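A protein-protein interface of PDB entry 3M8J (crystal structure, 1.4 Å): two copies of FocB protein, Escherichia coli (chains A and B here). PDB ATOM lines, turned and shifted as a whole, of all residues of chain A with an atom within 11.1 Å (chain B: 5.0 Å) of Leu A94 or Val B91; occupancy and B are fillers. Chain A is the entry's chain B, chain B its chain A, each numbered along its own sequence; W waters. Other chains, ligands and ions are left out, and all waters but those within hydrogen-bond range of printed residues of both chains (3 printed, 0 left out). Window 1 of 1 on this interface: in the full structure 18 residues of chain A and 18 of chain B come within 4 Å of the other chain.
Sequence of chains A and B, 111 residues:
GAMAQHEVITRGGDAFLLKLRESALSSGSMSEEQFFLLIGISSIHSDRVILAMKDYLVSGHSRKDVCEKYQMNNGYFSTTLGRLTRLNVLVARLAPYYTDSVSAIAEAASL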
ATOM      1  N   GLU A  33     -18.983 -32.323 -17.981  1.00  0.00           N
ATOM      2  CA  GLU A  33     -19.968 -32.306 -16.931  1.00  0.00           C
ATOM      3  C   GLU A  33     -20.210 -30.903 -16.383  1.00  0.00           C
ATOM      4  O   GLU A  33     -21.325 -30.543 -16.066  1.00  0.00           O
ATOM      5  CB  GLU A  33     -19.598 -33.315 -15.842  1.00  0.00           C
ATOM      6  CG  GLU A  33     -19.540 -34.761 -16.370  1.00  0.00           C
ATOM      7  CD  GLU A  33     -18.178 -35.186 -16.979  1.00  0.00           C
ATOM      8  OE1 GLU A  33     -17.264 -34.361 -17.198  1.00  0.00           O
ATOM      9  OE2 GLU A  33     -18.021 -36.408 -17.227  1.00  0.00           O
ATOM     10  N   GLN A  34     -19.140 -30.118 -16.275  1.00  0.00           N
ATOM     11  CA  GLN A  34     -19.300 -28.726 -15.888  1.00  0.00           C
ATOM     12  C   GLN A  34     -20.194 -27.971 -16.905  1.00  0.00           C
ATOM     13  O   GLN A  34     -21.120 -27.244 -16.535  1.00  0.00           O
ATOM     14  CB  GLN A  34     -17.933 -28.038 -15.762  1.00  0.00           C
ATOM     15  CG  GLN A  34     -18.093 -26.582 -15.347  1.00  0.00           C
ATOM     16  CD  GLN A  34     -16.804 -25.809 -15.346  1.00  0.00           C
ATOM     17  OE1 GLN A  34     -15.739 -26.334 -15.619  1.00  0.00           O
ATOM     18  NE2 GLN A  34     -16.890 -24.555 -15.018  1.00  0.00           N
ATOM     19  N   PHE A  36     -22.459 -29.252 -18.939  1.00  0.00           N
ATOM     20  CA  PHE A  36     -23.839 -29.644 -18.814  1.00  0.00           C
ATOM     21  C   PHE A  36     -24.578 -29.095 -17.625  1.00  0.00           C
ATOM     22  O   PHE A  36     -25.787 -28.827 -17.700  1.00  0.00           O
ATOM     23  CB  PHE A  36     -24.031 -31.139 -19.003  1.00  0.00           C
ATOM     24  CG  PHE A  36     -24.034 -31.503 -20.471  1.00  0.00           C
ATOM     25  CD1 PHE A  36     -24.998 -30.954 -21.330  1.00  0.00           C
ATOM     26  CD2 PHE A  36     -23.016 -32.267 -20.999  1.00  0.00           C
ATOM     27  CE1 PHE A  36     -24.988 -31.235 -22.690  1.00  0.00           C
ATOM     28  CE2 PHE A  36     -23.010 -32.580 -22.384  1.00  0.00           C
ATOM     29  CZ  PHE A  36     -23.992 -32.043 -23.212  1.00  0.00           C
ATOM     30  N   LEU A  37     -23.844 -28.916 -16.516  1.00  0.00           N
ATOM     31  CA  LEU A  37     -24.456 -28.256 -15.363  1.00  0.00           C
ATOM     32  C   LEU A  37     -24.780 -26.795 -15.682  1.00  0.00           C
ATOM     33  O   LEU A  37     -25.831 -26.297 -15.282  1.00  0.00           O
ATOM     34  CB  LEU A  37     -23.491 -28.345 -14.162  1.00  0.00           C
ATOM     35  CG  LEU A  37     -23.609 -29.641 -13.369  1.00  0.00           C
ATOM     36  CD1 LEU A  37     -22.303 -29.892 -12.534  1.00  0.00           C
ATOM     37  CD2 LEU A  37     -24.877 -29.660 -12.475  1.00  0.00           C
ATOM     38  N   LEU A  38     -23.858 -26.097 -16.390  1.00  0.00           N
ATOM     39  CA  LEU A  38     -24.149 -24.716 -16.780  1.00  0.00           C
ATOM     40  C   LEU A  38     -25.347 -24.642 -17.709  1.00  0.00           C
ATOM     41  O   LEU A  38     -26.184 -23.775 -17.577  1.00  0.00           O
ATOM     42  CB  LEU A  38     -22.912 -24.091 -17.432  1.00  0.00           C
ATOM     43  CG  LEU A  38     -21.775 -23.710 -16.500  1.00  0.00           C
ATOM     44  CD1 LEU A  38     -20.550 -23.304 -17.311  1.00  0.00           C
ATOM     45  CD2 LEU A  38     -22.237 -22.583 -15.537  1.00  0.00           C
ATOM     46  N   ILE A  39     -25.422 -25.566 -18.661  1.00  0.00           N
ATOM     47  CA  ILE A  39     -26.617 -25.629 -19.505  1.00  0.00           C
ATOM     48  C   ILE A  39     -27.884 -25.854 -18.670  1.00  0.00           C
ATOM     49  O   ILE A  39     -28.915 -25.220 -18.917  1.00  0.00           O
ATOM     50  CB  ILE A  39     -26.456 -26.683 -20.612  1.00  0.00           C
ATOM     51  CG1 ILE A  39     -25.363 -26.287 -21.603  1.00  0.00           C
ATOM     52  CG2 ILE A  39     -27.802 -26.906 -21.339  1.00  0.00           C
ATOM     53  CD1 ILE A  39     -25.554 -25.006 -22.396  1.00  0.00           C
ATOM     54  N   GLY A  40     -27.779 -26.739 -17.685  1.00  0.00           N
ATOM     55  CA  GLY A  40     -28.917 -27.056 -16.805  1.00  0.00           C
ATOM     56  C   GLY A  40     -29.455 -25.844 -16.081  1.00  0.00           C
ATOM     57  O   GLY A  40     -30.694 -25.674 -15.956  1.00  0.00           O
ATOM     58  N   ILE A  41     -28.572 -24.961 -15.629  1.00  0.00           N
ATOM     59  CA  ILE A  41     -28.995 -23.748 -14.928  1.00  0.00           C
ATOM     60  C   ILE A  41     -29.466 -22.690 -15.863  1.00  0.00           C
ATOM     61  O   ILE A  41     -30.226 -21.797 -15.449  1.00  0.00           O
ATOM     62  CB  ILE A  41     -27.981 -23.216 -13.913  1.00  0.00           C
ATOM     63  CG1 ILE A  41     -26.666 -22.863 -14.540  1.00  0.00           C
ATOM     64  CG2 ILE A  41     -27.792 -24.219 -12.833  1.00  0.00           C
ATOM     65  CD1 ILE A  41     -25.782 -22.063 -13.572  1.00  0.00           C
ATOM     66  N   SER A  42     -29.072 -22.780 -17.130  1.00  0.00           N
ATOM     67  CA  SER A  42     -29.392 -21.772 -18.121  1.00  0.00           C
ATOM     68  C   SER A  42     -30.800 -21.891 -18.624  1.00  0.00           C
ATOM     69  O   SER A  42     -31.488 -22.891 -18.372  1.00  0.00           O
ATOM     70  CB  SER A  42     -28.434 -21.898 -19.318  1.00  0.00           C
ATOM     71  OG  SER A  42     -28.906 -22.871 -20.253  1.00  0.00           O
ATOM     72  N   THR A  85     -21.073 -17.076 -20.629  1.00  0.00           N
ATOM     73  CA  THR A  85     -20.060 -16.319 -19.877  1.00  0.00           C
ATOM     74  C   THR A  85     -20.742 -15.680 -18.694  1.00  0.00           C
ATOM     75  O   THR A  85     -20.180 -15.731 -17.601  1.00  0.00           O
ATOM     76  CB  THR A  85     -19.458 -15.252 -20.768  1.00  0.00           C
ATOM     77  OG1 THR A  85     -18.701 -15.902 -21.783  1.00  0.00           O
ATOM     78  CG2 THR A  85     -18.558 -14.318 -19.991  1.00  0.00           C
ATOM     79  N   ARG A  86     -21.918 -15.068 -18.880  1.00  0.00           N
ATOM     80  CA  ARG A  86     -22.619 -14.429 -17.755  1.00  0.00           C
ATOM     81  C   ARG A  86     -22.871 -15.438 -16.650  1.00  0.00           C
ATOM     82  O   ARG A  86     -22.637 -15.176 -15.479  1.00  0.00           O
ATOM     83  CB  ARG A  86     -23.886 -13.753 -18.243  1.00  0.00           C
ATOM     84  CG  ARG A  86     -24.717 -13.147 -17.116  1.00  0.00           C
ATOM     85  CD  ARG A  86     -25.988 -12.535 -17.601  1.00  0.00           C
ATOM     86  NE  ARG A  86     -26.862 -12.233 -16.462  1.00  0.00           N
ATOM     87  CZ  ARG A  86     -27.732 -13.115 -15.932  1.00  0.00           C
ATOM     88  NH1 ARG A  86     -27.956 -14.268 -16.520  1.00  0.00           N
ATOM     89  NH2 ARG A  86     -28.435 -12.766 -14.905  1.00  0.00           N
ATOM     90  N   LEU A  87     -23.416 -16.599 -17.043  1.00  0.00           N
ATOM     91  CA  LEU A  87     -23.715 -17.595 -16.007  1.00  0.00           C
ATOM     92  C   LEU A  87     -22.449 -18.057 -15.311  1.00  0.00           C
ATOM     93  O   LEU A  87     -22.423 -18.233 -14.076  1.00  0.00           O
ATOM     94  CB  LEU A  87     -24.412 -18.799 -16.629  1.00  0.00           C
ATOM     95  CG  LEU A  87     -25.832 -18.451 -17.040  1.00  0.00           C
ATOM     96  CD1 LEU A  87     -26.351 -19.579 -17.943  1.00  0.00           C
ATOM     97  CD2 LEU A  87     -26.767 -18.270 -15.827  1.00  0.00           C
ATOM     98  N   ASN A  88     -21.360 -18.254 -16.042  1.00  0.00           N
ATOM     99  CA  ASN A  88     -20.109 -18.687 -15.454  1.00  0.00           C
ATOM    100  C   ASN A  88     -19.571 -17.672 -14.451  1.00  0.00           C
ATOM    101  O   ASN A  88     -19.062 -18.076 -13.390  1.00  0.00           O
ATOM    102  CB  ASN A  88     -19.049 -18.934 -16.568  1.00  0.00           C
ATOM    103  CG  ASN A  88     -17.742 -19.489 -16.023  1.00  0.00           C
ATOM    104  OD1 ASN A  88     -16.754 -18.762 -15.947  1.00  0.00           O
ATOM    105  ND2 ASN A  88     -17.733 -20.739 -15.605  1.00  0.00           N
ATOM    106  N   VAL A  89     -19.706 -16.374 -14.746  1.00  0.00           N
ATOM    107  CA  VAL A  89     -19.231 -15.333 -13.795  1.00  0.00           C
ATOM    108  C   VAL A  89     -20.070 -15.431 -12.521  1.00  0.00           C
ATOM    109  O   VAL A  89     -19.528 -15.361 -11.404  1.00  0.00           O
ATOM    110  CB  VAL A  89     -19.458 -13.940 -14.403  1.00  0.00           C
ATOM    111  CG1 VAL A  89     -19.265 -12.827 -13.332  1.00  0.00           C
ATOM    112  CG2 VAL A  89     -18.489 -13.734 -15.577  1.00  0.00           C
ATOM    113  N   LEU A  90     -21.385 -15.606 -12.652  1.00  0.00           N
ATOM    114  CA  LEU A  90     -22.230 -15.684 -11.466  1.00  0.00           C
ATOM    115  C   LEU A  90     -21.934 -16.925 -10.647  1.00  0.00           C
ATOM    116  O   LEU A  90     -21.855 -16.840  -9.426  1.00  0.00           O
ATOM    117  CB  LEU A  90     -23.710 -15.647 -11.905  1.00  0.00           C
ATOM    118  CG  LEU A  90     -24.143 -14.351 -12.618  1.00  0.00           C
ATOM    119  CD1 LEU A  90     -25.590 -14.549 -13.104  1.00  0.00           C
ATOM    120  CD2 LEU A  90     -23.975 -13.103 -11.709  1.00  0.00           C
ATOM    121  N   VAL A  91     -21.746 -18.051 -11.310  1.00  0.00           N
ATOM    122  CA  VAL A  91     -21.399 -19.271 -10.601  1.00  0.00           C
ATOM    123  C   VAL A  91     -20.031 -19.162  -9.918  1.00  0.00           C
ATOM    124  O   VAL A  91     -19.905 -19.592  -8.781  1.00  0.00           O
ATOM    125  CB  VAL A  91     -21.474 -20.488 -11.562  1.00  0.00           C
ATOM    126  CG1 VAL A  91     -20.947 -21.735 -10.870  1.00  0.00           C
ATOM    127  CG2 VAL A  91     -22.908 -20.700 -12.002  1.00  0.00           C
ATOM    128  N   ALA A  92     -19.045 -18.549 -10.567  1.00  0.00           N
ATOM    129  CA  ALA A  92     -17.748 -18.384  -9.930  1.00  0.00           C
ATOM    130  C   ALA A  92     -17.889 -17.514  -8.694  1.00  0.00           C
ATOM    131  O   ALA A  92     -17.234 -17.798  -7.699  1.00  0.00           O
ATOM    132  CB  ALA A  92     -16.769 -17.758 -10.926  1.00  0.00           C
ATOM    133  N   ARG A  93     -18.704 -16.450  -8.760  1.00  0.00           N
ATOM    134  CA  ARG A  93     -18.930 -15.618  -7.589  1.00  0.00           C
ATOM    135  C   ARG A  93     -19.692 -16.355  -6.502  1.00  0.00           C
ATOM    136  O   ARG A  93     -19.501 -16.097  -5.311  1.00  0.00           O
ATOM    137  CB  ARG A  93     -19.669 -14.356  -8.010  1.00  0.00           C
ATOM    138  CG  ARG A  93     -18.767 -13.396  -8.772  1.00  0.00           C
ATOM    139  CD  ARG A  93     -19.546 -12.215  -9.288  1.00  0.00           C
ATOM    140  NE  ARG A  93     -20.026 -11.373  -8.197  1.00  0.00           N
ATOM    141  CZ  ARG A  93     -20.772 -10.286  -8.375  1.00  0.00           C
ATOM    142  NH1 ARG A  93     -21.110  -9.883  -9.598  1.00  0.00           N
ATOM    143  NH2 ARG A  93     -21.184  -9.606  -7.319  1.00  0.00           N
ATOM    144  N   LEU A  94     -20.554 -17.301  -6.875  1.00  0.00           N
ATOM    145  CA  LEU A  94     -21.248 -18.075  -5.867  1.00  0.00           C
ATOM    146  C   LEU A  94     -20.373 -19.135  -5.218  1.00  0.00           C
ATOM    147  O   LEU A  94     -20.609 -19.487  -4.058  1.00  0.00           O
ATOM    148  CB  LEU A  94     -22.484 -18.730  -6.515  1.00  0.00           C
ATOM    149  CG  LEU A  94     -23.695 -17.822  -6.610  1.00  0.00           C
ATOM    150  CD1 LEU A  94     -24.667 -18.401  -7.660  1.00  0.00           C
ATOM    151  CD2 LEU A  94     -24.352 -17.785  -5.246  1.00  0.00           C
ATOM    152  N   ALA A  95     -19.384 -19.645  -5.959  1.00  0.00           N
ATOM    153  CA  ALA A  95     -18.633 -20.816  -5.464  1.00  0.00           C
ATOM    154  C   ALA A  95     -18.096 -20.732  -4.033  1.00  0.00           C
ATOM    155  O   ALA A  95     -18.240 -21.742  -3.334  1.00  0.00           O
ATOM    156  CB  ALA A  95     -17.517 -21.259  -6.461  1.00  0.00           C
ATOM    157  N   PRO A  96     -17.567 -19.567  -3.592  1.00  0.00           N
ATOM    158  CA  PRO A  96     -17.015 -19.544  -2.234  1.00  0.00           C
ATOM    159  C   PRO A  96     -18.069 -19.747  -1.158  1.00  0.00           C
ATOM    160  O   PRO A  96     -17.740 -20.143  -0.031  1.00  0.00           O
ATOM    161  CB  PRO A  96     -16.465 -18.113  -2.127  1.00  0.00           C
ATOM    162  CG  PRO A  96     -16.105 -17.757  -3.515  1.00  0.00           C
ATOM    163  CD  PRO A  96     -17.196 -18.372  -4.368  1.00  0.00           C
ATOM    164  N   TYR A  97     -19.363 -19.555  -1.450  1.00  0.00           N
ATOM    165  CA  TYR A  97     -20.407 -19.882  -0.472  1.00  0.00           C
ATOM    166  C   TYR A  97     -20.670 -21.373  -0.302  1.00  0.00           C
ATOM    167  O   TYR A  97     -21.469 -21.776   0.578  1.00  0.00           O
ATOM    168  CB  TYR A  97     -21.720 -19.187  -0.856  1.00  0.00           C
ATOM    169  CG  TYR A  97     -21.649 -17.686  -0.846  1.00  0.00           C
ATOM    170  CD1 TYR A  97     -21.808 -16.980   0.347  1.00  0.00           C
ATOM    171  CD2 TYR A  97     -21.425 -16.961  -2.009  1.00  0.00           C
ATOM    172  CE1 TYR A  97     -21.734 -15.608   0.346  1.00  0.00           C
ATOM    173  CE2 TYR A  97     -21.344 -15.579  -2.033  1.00  0.00           C
ATOM    174  CZ  TYR A  97     -21.521 -14.905  -0.830  1.00  0.00           C
ATOM    175  OH  TYR A  97     -21.425 -13.514  -0.865  1.00  0.00           O
ATOM    176  N   TYR A  98     -20.048 -22.229  -1.141  1.00  0.00           N
ATOM    177  CA  TYR A  98     -20.322 -23.657  -1.150  1.00  0.00           C
ATOM    178  C   TYR A  98     -19.081 -24.497  -0.862  1.00  0.00           C
ATOM    179  O   TYR A  98     -19.204 -25.698  -0.637  1.00  0.00           O
ATOM    180  CB  TYR A  98     -20.906 -24.068  -2.496  1.00  0.00           C
ATOM    181  CG  TYR A  98     -22.198 -23.372  -2.765  1.00  0.00           C
ATOM    182  CD1 TYR A  98     -22.226 -22.169  -3.395  1.00  0.00           C
ATOM    183  CD2 TYR A  98     -23.407 -23.929  -2.360  1.00  0.00           C
ATOM    184  CE1 TYR A  98     -23.414 -21.494  -3.613  1.00  0.00           C
ATOM    185  CE2 TYR A  98     -24.634 -23.270  -2.616  1.00  0.00           C
ATOM    186  CZ  TYR A  98     -24.611 -22.047  -3.246  1.00  0.00           C
ATOM    187  OH  TYR A  98     -25.771 -21.347  -3.472  1.00  0.00           O
ATOM    188  N   THR A  99     -17.905 -23.865  -0.831  1.00  0.00           N
ATOM    189  CA  THR A  99     -16.632 -24.609  -0.771  1.00  0.00           C
ATOM    190  C   THR A  99     -15.981 -24.708   0.607  1.00  0.00           C
ATOM    191  O   THR A  99     -14.737 -24.690   0.695  1.00  0.00           O
ATOM    192  CB  THR A  99     -15.597 -23.941  -1.650  1.00  0.00           C
ATOM    193  OG1 THR A  99     -15.394 -22.601  -1.163  1.00  0.00           O
ATOM    194  CG2 THR A  99     -16.042 -23.989  -3.174  1.00  0.00           C
ATOM    195  N   GLN B  34     -25.202 -13.320  -2.018  1.00  0.00           N
ATOM    196  CA  GLN B  34     -25.515 -14.715  -2.446  1.00  0.00           C
ATOM    197  C   GLN B  34     -26.914 -14.798  -3.068  1.00  0.00           C
ATOM    198  O   GLN B  34     -27.123 -15.408  -4.114  1.00  0.00           O
ATOM    199  CB  GLN B  34     -25.365 -15.728  -1.320  1.00  0.00           C
ATOM    200  CG  GLN B  34     -25.656 -17.144  -1.786  1.00  0.00           C
ATOM    201  CD  GLN B  34     -25.468 -18.216  -0.736  1.00  0.00           C
ATOM    202  OE1 GLN B  34     -25.282 -17.944   0.451  1.00  0.00           O
ATOM    203  NE2 GLN B  34     -25.504 -19.441  -1.176  1.00  0.00           N
ATOM    204  N   LEU B  37     -27.030 -13.173  -6.570  1.00  0.00           N
ATOM    205  CA  LEU B  37     -26.380 -14.060  -7.522  1.00  0.00           C
ATOM    206  C   LEU B  37     -27.278 -15.228  -7.932  1.00  0.00           C
ATOM    207  O   LEU B  37     -27.357 -15.541  -9.134  1.00  0.00           O
ATOM    208  CB  LEU B  37     -25.070 -14.592  -6.952  1.00  0.00           C
ATOM    209  CG  LEU B  37     -23.969 -13.539  -6.739  1.00  0.00           C
ATOM    210  CD1 LEU B  37     -22.823 -14.083  -5.930  1.00  0.00           C
ATOM    211  CD2 LEU B  37     -23.470 -13.072  -8.102  1.00  0.00           C
ATOM    212  N   LEU B  38     -27.975 -15.863  -6.976  1.00  0.00           N
ATOM    213  CA  LEU B  38     -28.907 -16.911  -7.324  1.00  0.00           C
ATOM    214  C   LEU B  38     -30.057 -16.369  -8.157  1.00  0.00           C
ATOM    215  O   LEU B  38     -30.471 -16.990  -9.141  1.00  0.00           O
ATOM    216  CB  LEU B  38     -29.442 -17.635  -6.092  1.00  0.00           C
ATOM    217  CG  LEU B  38     -28.435 -18.499  -5.384  1.00  0.00           C
ATOM    218  CD1 LEU B  38     -28.959 -18.915  -4.037  1.00  0.00           C
ATOM    219  CD2 LEU B  38     -28.161 -19.760  -6.232  1.00  0.00           C
ATOM    220  N   ILE B  41     -28.930 -15.916 -11.766  1.00  0.00           N
ATOM    221  CA  ILE B  41     -28.907 -17.155 -12.585  1.00  0.00           C
ATOM    222  C   ILE B  41     -30.326 -17.588 -12.934  1.00  0.00           C
ATOM    223  O   ILE B  41     -30.568 -18.138 -14.021  1.00  0.00           O
ATOM    224  CB  ILE B  41     -28.195 -18.284 -11.849  1.00  0.00           C
ATOM    225  CG1 ILE B  41     -26.697 -17.971 -11.662  1.00  0.00           C
ATOM    226  CG2 ILE B  41     -28.554 -19.694 -12.478  1.00  0.00           C
ATOM    227  CD1 ILE B  41     -26.112 -18.963 -10.726  1.00  0.00           C
ATOM    228  N   LEU B  87     -31.802 -24.345  -7.899  1.00  0.00           N
ATOM    229  CA  LEU B  87     -30.561 -23.656  -8.338  1.00  0.00           C
ATOM    230  C   LEU B  87     -29.492 -23.764  -7.301  1.00  0.00           C
ATOM    231  O   LEU B  87     -28.314 -23.949  -7.637  1.00  0.00           O
ATOM    232  CB  LEU B  87     -30.860 -22.199  -8.666  1.00  0.00           C
ATOM    233  CG  LEU B  87     -31.731 -22.036  -9.905  1.00  0.00           C
ATOM    234  CD1 LEU B  87     -32.202 -20.608 -10.063  1.00  0.00           C
ATOM    235  CD2 LEU B  87     -30.998 -22.427 -11.188  1.00  0.00           C
ATOM    236  N   ASN B  88     -29.847 -23.676  -6.030  1.00  0.00           N
ATOM    237  CA  ASN B  88     -28.865 -23.820  -4.992  1.00  0.00           C
ATOM    238  C   ASN B  88     -28.192 -25.191  -5.028  1.00  0.00           C
ATOM    239  O   ASN B  88     -26.968 -25.287  -4.883  1.00  0.00           O
ATOM    240  CB  ASN B  88     -29.546 -23.615  -3.616  1.00  0.00           C
ATOM    241  CG  ASN B  88     -28.576 -23.592  -2.466  1.00  0.00           C
ATOM    242  OD1 ASN B  88     -28.526 -24.536  -1.665  1.00  0.00           O
ATOM    243  ND2 ASN B  88     -27.803 -22.555  -2.363  1.00  0.00           N
ATOM    244  N   VAL B  89     -28.960 -26.247  -5.225  1.00  0.00           N
ATOM    245  CA  VAL B  89     -28.391 -27.605  -5.328  1.00  0.00           C
ATOM    246  C   VAL B  89     -27.447 -27.671  -6.530  1.00  0.00           C
ATOM    247  O   VAL B  89     -26.343 -28.233  -6.457  1.00  0.00           O
ATOM    248  CB  VAL B  89     -29.522 -28.630  -5.516  1.00  0.00           C
ATOM    249  CG1 VAL B  89     -28.919 -30.019  -5.834  1.00  0.00           C
ATOM    250  CG2 VAL B  89     -30.310 -28.764  -4.212  1.00  0.00           C
ATOM    251  N   LEU B  90     -27.870 -27.168  -7.683  1.00  0.00           N
ATOM    252  CA  LEU B  90     -27.037 -27.220  -8.885  1.00  0.00           C
ATOM    253  C   LEU B  90     -25.769 -26.401  -8.782  1.00  0.00           C
ATOM    254  O   LEU B  90     -24.687 -26.849  -9.240  1.00  0.00           O
ATOM    255  CB  LEU B  90     -27.830 -26.817 -10.139  1.00  0.00           C
ATOM    256  CG  LEU B  90     -28.981 -27.814 -10.406  1.00  0.00           C
ATOM    257  CD1 LEU B  90     -29.772 -27.344 -11.609  1.00  0.00           C
ATOM    258  CD2 LEU B  90     -28.517 -29.319 -10.587  1.00  0.00           C
ATOM    259  N   VAL B  91     -25.850 -25.227  -8.167  1.00  0.00           N
ATOM    260  CA  VAL B  91     -24.671 -24.421  -7.971  1.00  0.00           C
ATOM    261  C   VAL B  91     -23.690 -25.108  -7.009  1.00  0.00           C
ATOM    262  O   VAL B  91     -22.467 -25.066  -7.242  1.00  0.00           O
ATOM    263  CB  VAL B  91     -25.077 -23.019  -7.465  1.00  0.00           C
ATOM    264  CG1 VAL B  91     -23.815 -22.246  -6.985  1.00  0.00           C
ATOM    265  CG2 VAL B  91     -25.805 -22.256  -8.575  1.00  0.00           C
ATOM    266  N   ALA B  92     -24.205 -25.778  -5.987  1.00  0.00           N
ATOM    267  CA  ALA B  92     -23.320 -26.506  -5.095  1.00  0.00           C
ATOM    268  C   ALA B  92     -22.602 -27.614  -5.848  1.00  0.00           C
ATOM    269  O   ALA B  92     -21.420 -27.889  -5.542  1.00  0.00           O
ATOM    270  CB  ALA B  92     -24.137 -27.094  -3.903  1.00  0.00           C
ATOM    271  N   ARG B  93     -23.270 -28.266  -6.811  1.00  0.00           N
ATOM    272  CA  ARG B  93     -22.614 -29.295  -7.635  1.00  0.00           C
ATOM    273  C   ARG B  93     -21.618 -28.707  -8.621  1.00  0.00           C
ATOM    274  O   ARG B  93     -20.642 -29.386  -8.978  1.00  0.00           O
ATOM    275  CB  ARG B  93     -23.643 -30.106  -8.360  1.00  0.00           C
ATOM    276  CG  ARG B  93     -24.452 -30.965  -7.444  1.00  0.00           C
ATOM    277  CD  ARG B  93     -25.457 -31.765  -8.206  1.00  0.00           C
ATOM    278  NE  ARG B  93     -26.284 -32.476  -7.257  1.00  0.00           N
ATOM    279  CZ  ARG B  93     -27.417 -33.061  -7.587  1.00  0.00           C
ATOM    280  NH1 ARG B  93     -27.831 -33.043  -8.847  1.00  0.00           N
ATOM    281  NH2 ARG B  93     -28.115 -33.683  -6.654  1.00  0.00           N
ATOM    282  N   LEU B  94     -21.798 -27.433  -9.025  1.00  0.00           N
ATOM    283  CA  LEU B  94     -20.843 -26.779  -9.893  1.00  0.00           C
ATOM    284  C   LEU B  94     -19.603 -26.268  -9.141  1.00  0.00           C
ATOM    285  O   LEU B  94     -18.532 -26.184  -9.735  1.00  0.00           O
ATOM    286  CB  LEU B  94     -21.521 -25.569 -10.566  1.00  0.00           C
ATOM    287  CG  LEU B  94     -22.164 -25.904 -11.885  1.00  0.00           C
ATOM    288  CD1 LEU B  94     -23.201 -24.865 -12.211  1.00  0.00           C
ATOM    289  CD2 LEU B  94     -21.095 -25.959 -12.954  1.00  0.00           C
ATOM    290  N   ALA B  95     -19.755 -25.911  -7.860  1.00  0.00           N
ATOM    291  CA  ALA B  95     -18.714 -25.227  -7.153  1.00  0.00           C
ATOM    292  C   ALA B  95     -17.343 -25.904  -7.188  1.00  0.00           C
ATOM    293  O   ALA B  95     -16.359 -25.195  -7.303  1.00  0.00           O
ATOM    294  CB  ALA B  95     -19.158 -24.901  -5.723  1.00  0.00           C
HETATM  295  O   HOH W   1     -31.645 -19.621 -15.730  1.00  0.00           O
HETATM  296  O   HOH W   2     -19.972 -27.652  -3.258  1.00  0.00           O
HETATM  297  O   HOH W   3     -30.762 -15.667 -16.125  1.00  0.00           O
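The side-chain amide nitrogen (NE2) of Gln B34 is in hydrogen-bond range of the side-chain hydroxyl (OH) of Tyr A98, 3.0 Å away.
The side-chain hydroxyl (OH) of Tyr A98 is in hydrogen-bond range of the side-chain amide nitrogen (ND2) of Asn B88 (2.6 Å).
Leu A37 touches Arg B93 (CD1 to O, 3.96 Å).
CB of Leu A90 touches CG1 of Ile B41, at 3.8 Å.
Val A91 touches Ile B41.
Val A91 touches Leu B94.
Leu A94 touches Gln B34 (CD2 to CG, 3.8 Å).
Leu B37 touches Leu A94 (CB to CG, 3.5 Å).
Leu A94 touches Val B91.
Tyr A98 touches Leu B38 (OH to CD2, 3.98 Å).
Tyr A98 touches Ala B92.
Ala B95 touches Tyr A98 (CB to CB, 3.8 Å).
Phe A36 touches none of the printed residues of chain B.
Of the printed residues of chain B, Leu A37 touches Arg B93 (3.96 Å) and Leu B94 (3.6 Å).
Of the printed residues of chain B, Val A91 touches Ile B41 (3.9 Å) and Leu B94 (3.9 Å).
Of the printed residues of chain B, Leu A94 touches Gln B34 (3.8 Å), Leu B37 (3.5 Å), Ile B41 (3.4 Å) and Val B91 (3.8 Å).
Ala A95 touches none of the printed residues of chain B.
Printed residues of chain B within 4 Å of Tyr A97: Gln B34.
Printed residues of chain B within 4 Å of Tyr A98: Gln B34, Leu B38, Asn B88, Val B91, Ala B92 and Ala B95.
Of chain A, only Leu A94, Tyr A97 and Tyr A98 come within 4 Å of Gln B34.
Of chain A, only Leu A90 (3.6 Å), Arg A93 (3.8 Å) and Leu A94 (3.5 Å) come within 4 Å of Leu B37.
No residue of chain A comes within 4 Å of Leu B87.
Of the printed residues of chain A, Asn B88 touches Tyr A98 (2.6 Å).
No residue of chain A comes within 4 Å of Val B89.
Val B91 touches just these residues of chain A: Leu A94 and Tyr A98.
Of the printed residues of chain A, Ala B92 touches Tyr A98 (3.6 Å).
Leu B94 touches just these residues of chain A: Gln A34 (3.8 Å), Leu A37 (3.6 Å) and Val A91 (3.9 Å).
Of the printed residues of chain A, Ala B95 touches Tyr A98 (3.8 Å).
The nearest printed residue of chain B that does not touch Leu A94 is Leu B38 (4.01 Å).
The nearest residue of chain A that does not touch Val B91 is Val A91 (4.7 Å).
Of the 24 printed residues of chain A, 9 touch a printed residue of chain B.
Hydrophobic or aromatic side chains of chain A within 4 Å of the printed part of chain B: Leu A37, Ile A41, Leu A90, Val A91, Leu A94, Tyr A97 and Tyr A98.
Along chain A the printed residues that touch a printed residue of chain B span positions 34 to 98.
Printed residues of chain B that touch a printed residue of chain A: Gln B34, Leu B37, Leu B38, Ile B41, Asn B88, Leu B90, Val B91, Ala B92, Arg B93, Leu B94 and Ala B95.
Hydrophobic or aromatic side chains of chain B within 4 Å of the printed part of chain A: Leu B37, Leu B38, Ile B41, Leu B90, Val B91, Ala B92, Leu B94 and Ala B95.
Among the printed residues, 21 pairs touch across the chains.
Among the printed residues, no Asp or Glu carboxylate lies within 4 Å of a Lys or Arg side-chain nitrogen of the other chain.
Ile A41 touches its own counterpart, Ile B41.
Ile A41 touches Leu B90, and with the chains exchanged Leu A90 touches Ile B41.
Leu A90 touches Leu B37, but with the chains exchanged Leu A37 does not touch Leu B90 (4.1 Å).
Val A91 touches Leu B94, and with the chains exchanged Leu A94 touches Val B91.
Positions printed for both chains: 34, 37, 38, 41, 87, 88, 89, 90, 91, 92, 93, 94 and 95.
Water W1 bridges the backbone carbonyl oxygen of Ile B41 and the backbone carbonyl oxygen of Ile A41.
Water W2 lies within hydrogen-bond range of O of Ala B92 (2.7 Å) and O of Tyr A98 (3.4 Å).
Water W3 bridges the guanidinium group (NH1) of Arg A86 (3.2 Å) and the backbone carbonyl oxygen (O) of Ile B41 (3.3 Å).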
